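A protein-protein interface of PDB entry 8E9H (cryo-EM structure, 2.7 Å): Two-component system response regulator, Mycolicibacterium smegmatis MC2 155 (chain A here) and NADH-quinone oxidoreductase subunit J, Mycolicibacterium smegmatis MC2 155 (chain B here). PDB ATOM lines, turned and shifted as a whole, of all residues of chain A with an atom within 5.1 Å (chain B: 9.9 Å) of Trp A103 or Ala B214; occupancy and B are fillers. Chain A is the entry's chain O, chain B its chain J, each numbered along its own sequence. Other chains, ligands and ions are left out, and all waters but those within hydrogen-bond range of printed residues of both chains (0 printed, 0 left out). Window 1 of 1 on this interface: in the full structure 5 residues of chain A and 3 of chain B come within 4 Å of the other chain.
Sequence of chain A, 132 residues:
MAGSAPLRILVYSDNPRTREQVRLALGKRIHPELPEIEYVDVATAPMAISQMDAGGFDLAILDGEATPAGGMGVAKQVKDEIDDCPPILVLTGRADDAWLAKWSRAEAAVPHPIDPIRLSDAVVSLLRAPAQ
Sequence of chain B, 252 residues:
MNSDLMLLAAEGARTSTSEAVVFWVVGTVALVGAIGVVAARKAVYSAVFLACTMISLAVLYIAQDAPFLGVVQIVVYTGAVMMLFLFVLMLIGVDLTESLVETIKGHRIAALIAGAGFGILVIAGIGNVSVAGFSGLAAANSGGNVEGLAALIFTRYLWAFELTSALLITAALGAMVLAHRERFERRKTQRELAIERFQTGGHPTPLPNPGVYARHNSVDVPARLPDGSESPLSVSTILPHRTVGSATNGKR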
ATOM      1  N   MET A  72      15.441   1.749   2.457  1.00  0.00           N
ATOM      2  CA  MET A  72      14.938   3.059   2.859  1.00  0.00           C
ATOM      3  C   MET A  72      13.999   2.942   4.051  1.00  0.00           C
ATOM      4  O   MET A  72      14.047   3.766   4.975  1.00  0.00           O
ATOM      5  CB  MET A  72      14.236   3.723   1.682  1.00  0.00           C
ATOM      6  CG  MET A  72      15.105   3.804   0.450  1.00  0.00           C
ATOM      7  SD  MET A  72      14.439   4.876  -0.825  1.00  0.00           S
ATOM      8  CE  MET A  72      14.531   3.790  -2.242  1.00  0.00           C
ATOM      9  N   GLY A  73      13.136   1.930   4.048  1.00  0.00           N
ATOM     10  CA  GLY A  73      12.281   1.711   5.198  1.00  0.00           C
ATOM     11  C   GLY A  73      13.083   1.441   6.454  1.00  0.00           C
ATOM     12  O   GLY A  73      12.771   1.956   7.528  1.00  0.00           O
ATOM     13  N   LYS A  76      14.598   4.752   7.710  1.00  0.00           N
ATOM     14  CA  LYS A  76      13.609   5.544   8.428  1.00  0.00           C
ATOM     15  C   LYS A  76      13.334   4.936   9.795  1.00  0.00           C
ATOM     16  O   LYS A  76      13.275   5.648  10.805  1.00  0.00           O
ATOM     17  CB  LYS A  76      12.327   5.635   7.603  1.00  0.00           C
ATOM     18  CG  LYS A  76      11.283   6.585   8.147  1.00  0.00           C
ATOM     19  CD  LYS A  76      11.715   8.027   7.998  1.00  0.00           C
ATOM     20  CE  LYS A  76      10.613   8.975   8.420  1.00  0.00           C
ATOM     21  NZ  LYS A  76      10.461   9.013   9.896  1.00  0.00           N
ATOM     22  N   TRP A  99      14.342  10.829  -4.401  1.00  0.00           N
ATOM     23  CA  TRP A  99      13.393  11.503  -3.526  1.00  0.00           C
ATOM     24  C   TRP A  99      13.162  10.703  -2.253  1.00  0.00           C
ATOM     25  O   TRP A  99      13.312  11.232  -1.147  1.00  0.00           O
ATOM     26  CB  TRP A  99      12.078  11.728  -4.262  1.00  0.00           C
ATOM     27  CG  TRP A  99      11.139  12.618  -3.535  1.00  0.00           C
ATOM     28  CD1 TRP A  99      11.160  13.977  -3.507  1.00  0.00           C
ATOM     29  CD2 TRP A  99      10.031  12.215  -2.731  1.00  0.00           C
ATOM     30  NE1 TRP A  99      10.133  14.448  -2.731  1.00  0.00           N
ATOM     31  CE2 TRP A  99       9.424  13.383  -2.243  1.00  0.00           C
ATOM     32  CE3 TRP A  99       9.493  10.978  -2.374  1.00  0.00           C
ATOM     33  CZ2 TRP A  99       8.307  13.353  -1.420  1.00  0.00           C
ATOM     34  CZ3 TRP A  99       8.386  10.951  -1.557  1.00  0.00           C
ATOM     35  CH2 TRP A  99       7.805  12.128  -1.088  1.00  0.00           C
ATOM     36  N   LEU A 100      12.836   9.416  -2.382  1.00  0.00           N
ATOM     37  CA  LEU A 100      12.655   8.608  -1.185  1.00  0.00           C
ATOM     38  C   LEU A 100      13.934   8.531  -0.373  1.00  0.00           C
ATOM     39  O   LEU A 100      13.879   8.488   0.860  1.00  0.00           O
ATOM     40  CB  LEU A 100      12.185   7.205  -1.545  1.00  0.00           C
ATOM     41  CG  LEU A 100      10.711   7.039  -1.896  1.00  0.00           C
ATOM     42  CD1 LEU A 100      10.417   5.589  -2.203  1.00  0.00           C
ATOM     43  CD2 LEU A 100       9.834   7.523  -0.765  1.00  0.00           C
ATOM     44  N   ALA A 101      15.092   8.516  -1.033  1.00  0.00           N
ATOM     45  CA  ALA A 101      16.342   8.527  -0.286  1.00  0.00           C
ATOM     46  C   ALA A 101      16.400   9.735   0.632  1.00  0.00           C
ATOM     47  O   ALA A 101      16.882   9.640   1.765  1.00  0.00           O
ATOM     48  CB  ALA A 101      17.530   8.519  -1.243  1.00  0.00           C
ATOM     49  N   LYS A 102      15.907  10.882   0.165  1.00  0.00           N
ATOM     50  CA  LYS A 102      15.812  12.045   1.037  1.00  0.00           C
ATOM     51  C   LYS A 102      14.814  11.796   2.156  1.00  0.00           C
ATOM     52  O   LYS A 102      15.071  12.120   3.319  1.00  0.00           O
ATOM     53  CB  LYS A 102      15.407  13.275   0.233  1.00  0.00           C
ATOM     54  CG  LYS A 102      16.482  13.780  -0.706  1.00  0.00           C
ATOM     55  CD  LYS A 102      16.038  15.009  -1.491  1.00  0.00           C
ATOM     56  CE  LYS A 102      15.393  16.068  -0.609  1.00  0.00           C
ATOM     57  NZ  LYS A 102      16.208  16.368   0.601  1.00  0.00           N
ATOM     58  N   TRP A 103      13.663  11.215   1.818  1.00  0.00           N
ATOM     59  CA  TRP A 103      12.646  10.963   2.829  1.00  0.00           C
ATOM     60  C   TRP A 103      13.169  10.029   3.905  1.00  0.00           C
ATOM     61  O   TRP A 103      12.849  10.187   5.087  1.00  0.00           O
ATOM     62  CB  TRP A 103      11.396  10.375   2.183  1.00  0.00           C
ATOM     63  CG  TRP A 103      10.535   9.675   3.162  1.00  0.00           C
ATOM     64  CD1 TRP A 103       9.623  10.240   3.995  1.00  0.00           C
ATOM     65  CD2 TRP A 103      10.507   8.273   3.427  1.00  0.00           C
ATOM     66  NE1 TRP A 103       9.023   9.278   4.761  1.00  0.00           N
ATOM     67  CE2 TRP A 103       9.550   8.060   4.431  1.00  0.00           C
ATOM     68  CE3 TRP A 103      11.199   7.176   2.914  1.00  0.00           C
ATOM     69  CZ2 TRP A 103       9.267   6.799   4.929  1.00  0.00           C
ATOM     70  CZ3 TRP A 103      10.915   5.926   3.409  1.00  0.00           C
ATOM     71  CH2 TRP A 103       9.960   5.746   4.407  1.00  0.00           C
ATOM     72  N   SER A 104      13.983   9.050   3.516  1.00  0.00           N
ATOM     73  CA  SER A 104      14.571   8.144   4.490  1.00  0.00           C
ATOM     74  C   SER A 104      15.518   8.854   5.439  1.00  0.00           C
ATOM     75  O   SER A 104      15.910   8.267   6.451  1.00  0.00           O
ATOM     76  CB  SER A 104      15.321   7.026   3.776  1.00  0.00           C
ATOM     77  OG  SER A 104      16.604   7.467   3.377  1.00  0.00           O
ATOM     78  N   ARG A 105      15.906  10.088   5.131  1.00  0.00           N
ATOM     79  CA  ARG A 105      16.819  10.864   5.959  1.00  0.00           C
ATOM     80  C   ARG A 105      18.192  10.219   6.046  1.00  0.00           C
ATOM     81  O   ARG A 105      18.985  10.556   6.927  1.00  0.00           O
ATOM     82  CB  ARG A 105      16.240  11.081   7.359  1.00  0.00           C
ATOM     83  CG  ARG A 105      15.148  12.126   7.386  1.00  0.00           C
ATOM     84  CD  ARG A 105      14.174  11.889   8.513  1.00  0.00           C
ATOM     85  NE  ARG A 105      13.200  12.967   8.613  1.00  0.00           N
ATOM     86  CZ  ARG A 105      12.074  13.031   7.918  1.00  0.00           C
ATOM     87  NH1 ARG A 105      11.760  12.109   7.022  1.00  0.00           N
ATOM     88  NH2 ARG A 105      11.242  14.047   8.122  1.00  0.00           N
ATOM     89  N   GLY B 211       2.730  22.490   0.425  1.00  0.00           N
ATOM     90  CA  GLY B 211       3.788  21.786  -0.273  1.00  0.00           C
ATOM     91  C   GLY B 211       4.095  20.452   0.386  1.00  0.00           C
ATOM     92  O   GLY B 211       4.076  20.327   1.606  1.00  0.00           O
ATOM     93  N   VAL B 212       4.366  19.454  -0.446  1.00  0.00           N
ATOM     94  CA  VAL B 212       4.745  18.125   0.009  1.00  0.00           C
ATOM     95  C   VAL B 212       6.191  17.906  -0.399  1.00  0.00           C
ATOM     96  O   VAL B 212       6.489  17.715  -1.584  1.00  0.00           O
ATOM     97  CB  VAL B 212       3.835  17.037  -0.571  1.00  0.00           C
ATOM     98  CG1 VAL B 212       4.330  15.669  -0.161  1.00  0.00           C
ATOM     99  CG2 VAL B 212       2.411  17.244  -0.106  1.00  0.00           C
ATOM    100  N   TYR B 213       7.088  17.935   0.575  1.00  0.00           N
ATOM    101  CA  TYR B 213       8.502  17.690   0.354  1.00  0.00           C
ATOM    102  C   TYR B 213       8.895  16.402   1.052  1.00  0.00           C
ATOM    103  O   TYR B 213       8.265  16.002   2.034  1.00  0.00           O
ATOM    104  CB  TYR B 213       9.362  18.835   0.889  1.00  0.00           C
ATOM    105  CG  TYR B 213       9.022  20.189   0.324  1.00  0.00           C
ATOM    106  CD1 TYR B 213       7.833  20.817   0.644  1.00  0.00           C
ATOM    107  CD2 TYR B 213       9.898  20.843  -0.523  1.00  0.00           C
ATOM    108  CE1 TYR B 213       7.522  22.053   0.132  1.00  0.00           C
ATOM    109  CE2 TYR B 213       9.593  22.079  -1.041  1.00  0.00           C
ATOM    110  CZ  TYR B 213       8.404  22.680  -0.708  1.00  0.00           C
ATOM    111  OH  TYR B 213       8.092  23.916  -1.219  1.00  0.00           O
ATOM    112  N   ALA B 214       9.930  15.746   0.543  1.00  0.00           N
ATOM    113  CA  ALA B 214      10.551  14.688   1.315  1.00  0.00           C
ATOM    114  C   ALA B 214      11.033  15.267   2.634  1.00  0.00           C
ATOM    115  O   ALA B 214      11.699  16.305   2.665  1.00  0.00           O
ATOM    116  CB  ALA B 214      11.717  14.073   0.544  1.00  0.00           C
ATOM    117  N   ARG B 215      10.685  14.600   3.726  1.00  0.00           N
ATOM    118  CA  ARG B 215      10.974  14.978   5.104  1.00  0.00           C
ATOM    119  C   ARG B 215       9.998  16.023   5.631  1.00  0.00           C
ATOM    120  O   ARG B 215      10.085  16.382   6.802  1.00  0.00           O
ATOM    121  CB  ARG B 215      12.406  15.507   5.295  1.00  0.00           C
ATOM    122  CG  ARG B 215      13.490  14.571   4.820  1.00  0.00           C
ATOM    123  CD  ARG B 215      14.859  15.141   5.112  1.00  0.00           C
ATOM    124  NE  ARG B 215      15.925  14.275   4.628  1.00  0.00           N
ATOM    125  CZ  ARG B 215      17.213  14.581   4.668  1.00  0.00           C
ATOM    126  NH1 ARG B 215      17.635  15.729   5.173  1.00  0.00           N
ATOM    127  NH2 ARG B 215      18.100  13.717   4.188  1.00  0.00           N
ATOM    128  N   HIS B 216       9.073  16.520   4.814  1.00  0.00           N
ATOM    129  CA  HIS B 216       8.152  17.559   5.268  1.00  0.00           C
ATOM    130  C   HIS B 216       6.885  17.492   4.437  1.00  0.00           C
ATOM    131  O   HIS B 216       6.920  17.775   3.238  1.00  0.00           O
ATOM    132  CB  HIS B 216       8.785  18.945   5.154  1.00  0.00           C
ATOM    133  CG  HIS B 216       9.997  19.131   6.007  1.00  0.00           C
ATOM    134  ND1 HIS B 216       9.939  19.163   7.382  1.00  0.00           N
ATOM    135  CD2 HIS B 216      11.299  19.304   5.680  1.00  0.00           C
ATOM    136  CE1 HIS B 216      11.154  19.340   7.868  1.00  0.00           C
ATOM    137  NE2 HIS B 216      11.998  19.429   6.856  1.00  0.00           N
ATOM    138  N   ASN B 217       5.771  17.129   5.069  1.00  0.00           N
ATOM    139  CA  ASN B 217       4.481  17.165   4.392  1.00  0.00           C
ATOM    140  C   ASN B 217       3.375  17.720   5.280  1.00  0.00           C
ATOM    141  O   ASN B 217       2.197  17.580   4.931  1.00  0.00           O
ATOM    142  CB  ASN B 217       4.095  15.771   3.893  1.00  0.00           C
ATOM    143  CG  ASN B 217       4.042  14.750   5.002  1.00  0.00           C
ATOM    144  OD1 ASN B 217       3.877  15.094   6.169  1.00  0.00           O
ATOM    145  ND2 ASN B 217       4.173  13.482   4.642  1.00  0.00           N
ATOM    146  N   SER B 218       3.707  18.346   6.404  1.00  0.00           N
ATOM    147  CA  SER B 218       2.689  18.930   7.258  1.00  0.00           C
ATOM    148  C   SER B 218       1.999  20.088   6.543  1.00  0.00           C
ATOM    149  O   SER B 218       2.457  20.576   5.509  1.00  0.00           O
ATOM    150  CB  SER B 218       3.307  19.417   8.565  1.00  0.00           C
ATOM    151  OG  SER B 218       4.443  20.220   8.310  1.00  0.00           O
ATOM    152  N   VAL B 221       3.944  23.451   5.818  1.00  0.00           N
ATOM    153  CA  VAL B 221       4.932  23.592   4.754  1.00  0.00           C
ATOM    154  C   VAL B 221       4.330  24.387   3.601  1.00  0.00           C
ATOM    155  O   VAL B 221       3.189  24.119   3.203  1.00  0.00           O
ATOM    156  CB  VAL B 221       5.417  22.219   4.270  1.00  0.00           C
ATOM    157  CG1 VAL B 221       6.456  22.385   3.193  1.00  0.00           C
ATOM    158  CG2 VAL B 221       5.974  21.415   5.427  1.00  0.00           C
ATOM    159  N   ARG B 224       5.863  25.257  -3.477  1.00  0.00           N
ATOM    160  CA  ARG B 224       6.931  25.906  -4.222  1.00  0.00           C
ATOM    161  C   ARG B 224       6.388  26.420  -5.550  1.00  0.00           C
ATOM    162  O   ARG B 224       5.825  25.650  -6.334  1.00  0.00           O
ATOM    163  CB  ARG B 224       8.082  24.932  -4.459  1.00  0.00           C
ATOM    164  CG  ARG B 224       9.246  25.521  -5.222  1.00  0.00           C
ATOM    165  CD  ARG B 224      10.418  24.565  -5.228  1.00  0.00           C
ATOM    166  NE  ARG B 224      10.998  24.415  -3.900  1.00  0.00           N
ATOM    167  CZ  ARG B 224      11.824  23.442  -3.546  1.00  0.00           C
ATOM    168  NH1 ARG B 224      12.194  22.503  -4.402  1.00  0.00           N
ATOM    169  NH2 ARG B 224      12.291  23.408  -2.302  1.00  0.00           N
ATOM    170  N   THR B 243       8.471  25.282   8.818  1.00  0.00           N
ATOM    171  CA  THR B 243       8.473  23.908   8.332  1.00  0.00           C
ATOM    172  C   THR B 243       8.867  23.855   6.862  1.00  0.00           C
ATOM    173  O   THR B 243       9.859  23.225   6.498  1.00  0.00           O
ATOM    174  CB  THR B 243       7.096  23.244   8.508  1.00  0.00           C
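O of Lys A102 is in hydrogen-bond range of NE of Arg B215 (2.7 Å). O of Arg B215 is in hydrogen-bond range of NH2 of Arg A105 (2.9 Å).
Trp A103 touches one residue of chain B. Ala B214 touches just these residues of chain A: Trp A99, Lys A102 and Trp A103. No residue of chain B comes within 4 Å of Gly A73. Leu A100 touches none of the printed residues of chain B. Ala A101 touches none of the printed residues of chain B. Lys A102 touches just these residues of chain B: Ala B214 (3.8 Å) and Arg B215 (2.7 Å). Of the printed residues of chain A, Arg B215 touches Lys A102 and Arg A105. Of the printed residues of chain A, Tyr B213 touches Trp A99 (3.97 Å). Of the printed residues of chain B, Trp A99 touches Tyr B213 and Ala B214. The nearest residue of chain B that does not touch Trp A103 is Arg B215 (4.2 Å). The nearest printed residue of chain A that does not touch Tyr B213 is Trp A103 (6.2 Å).
Trp A99 touches Tyr B213 (CZ2 to C, 3.97 Å). Trp A99 touches Ala B214 (CZ2 to N, 3.5 Å). CB of Lys A102 touches CB of Ala B214 (3.8 Å). Trp A103 touches Ala B214.
The backbone carbonyl oxygen (O) of Trp A103 is in hydrogen-bond range of the guanidinium group (NH1) of Arg A105 (2.9 Å). The side-chain hydroxyl (OH) of Tyr B213 lies close to the backbone NH (N) of Arg B224, 3.4 Å away.
Hydrophobic or aromatic side chains of chain B that line the printed part of chain A: Ala B214. Printed residues of chain A that touch a printed residue of chain B: Trp A99, Lys A102, Trp A103 and Arg A105. Hydrophobic or aromatic side chains of chain A within 4 Å of the printed part of chain B: Trp A99. Along chain A the printed residues that touch a printed residue of chain B span positions 99 to 105. Among the printed residues, no Asp or Glu carboxylate lies within 4 Å of a Lys or Arg side-chain nitrogen of the other chain.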
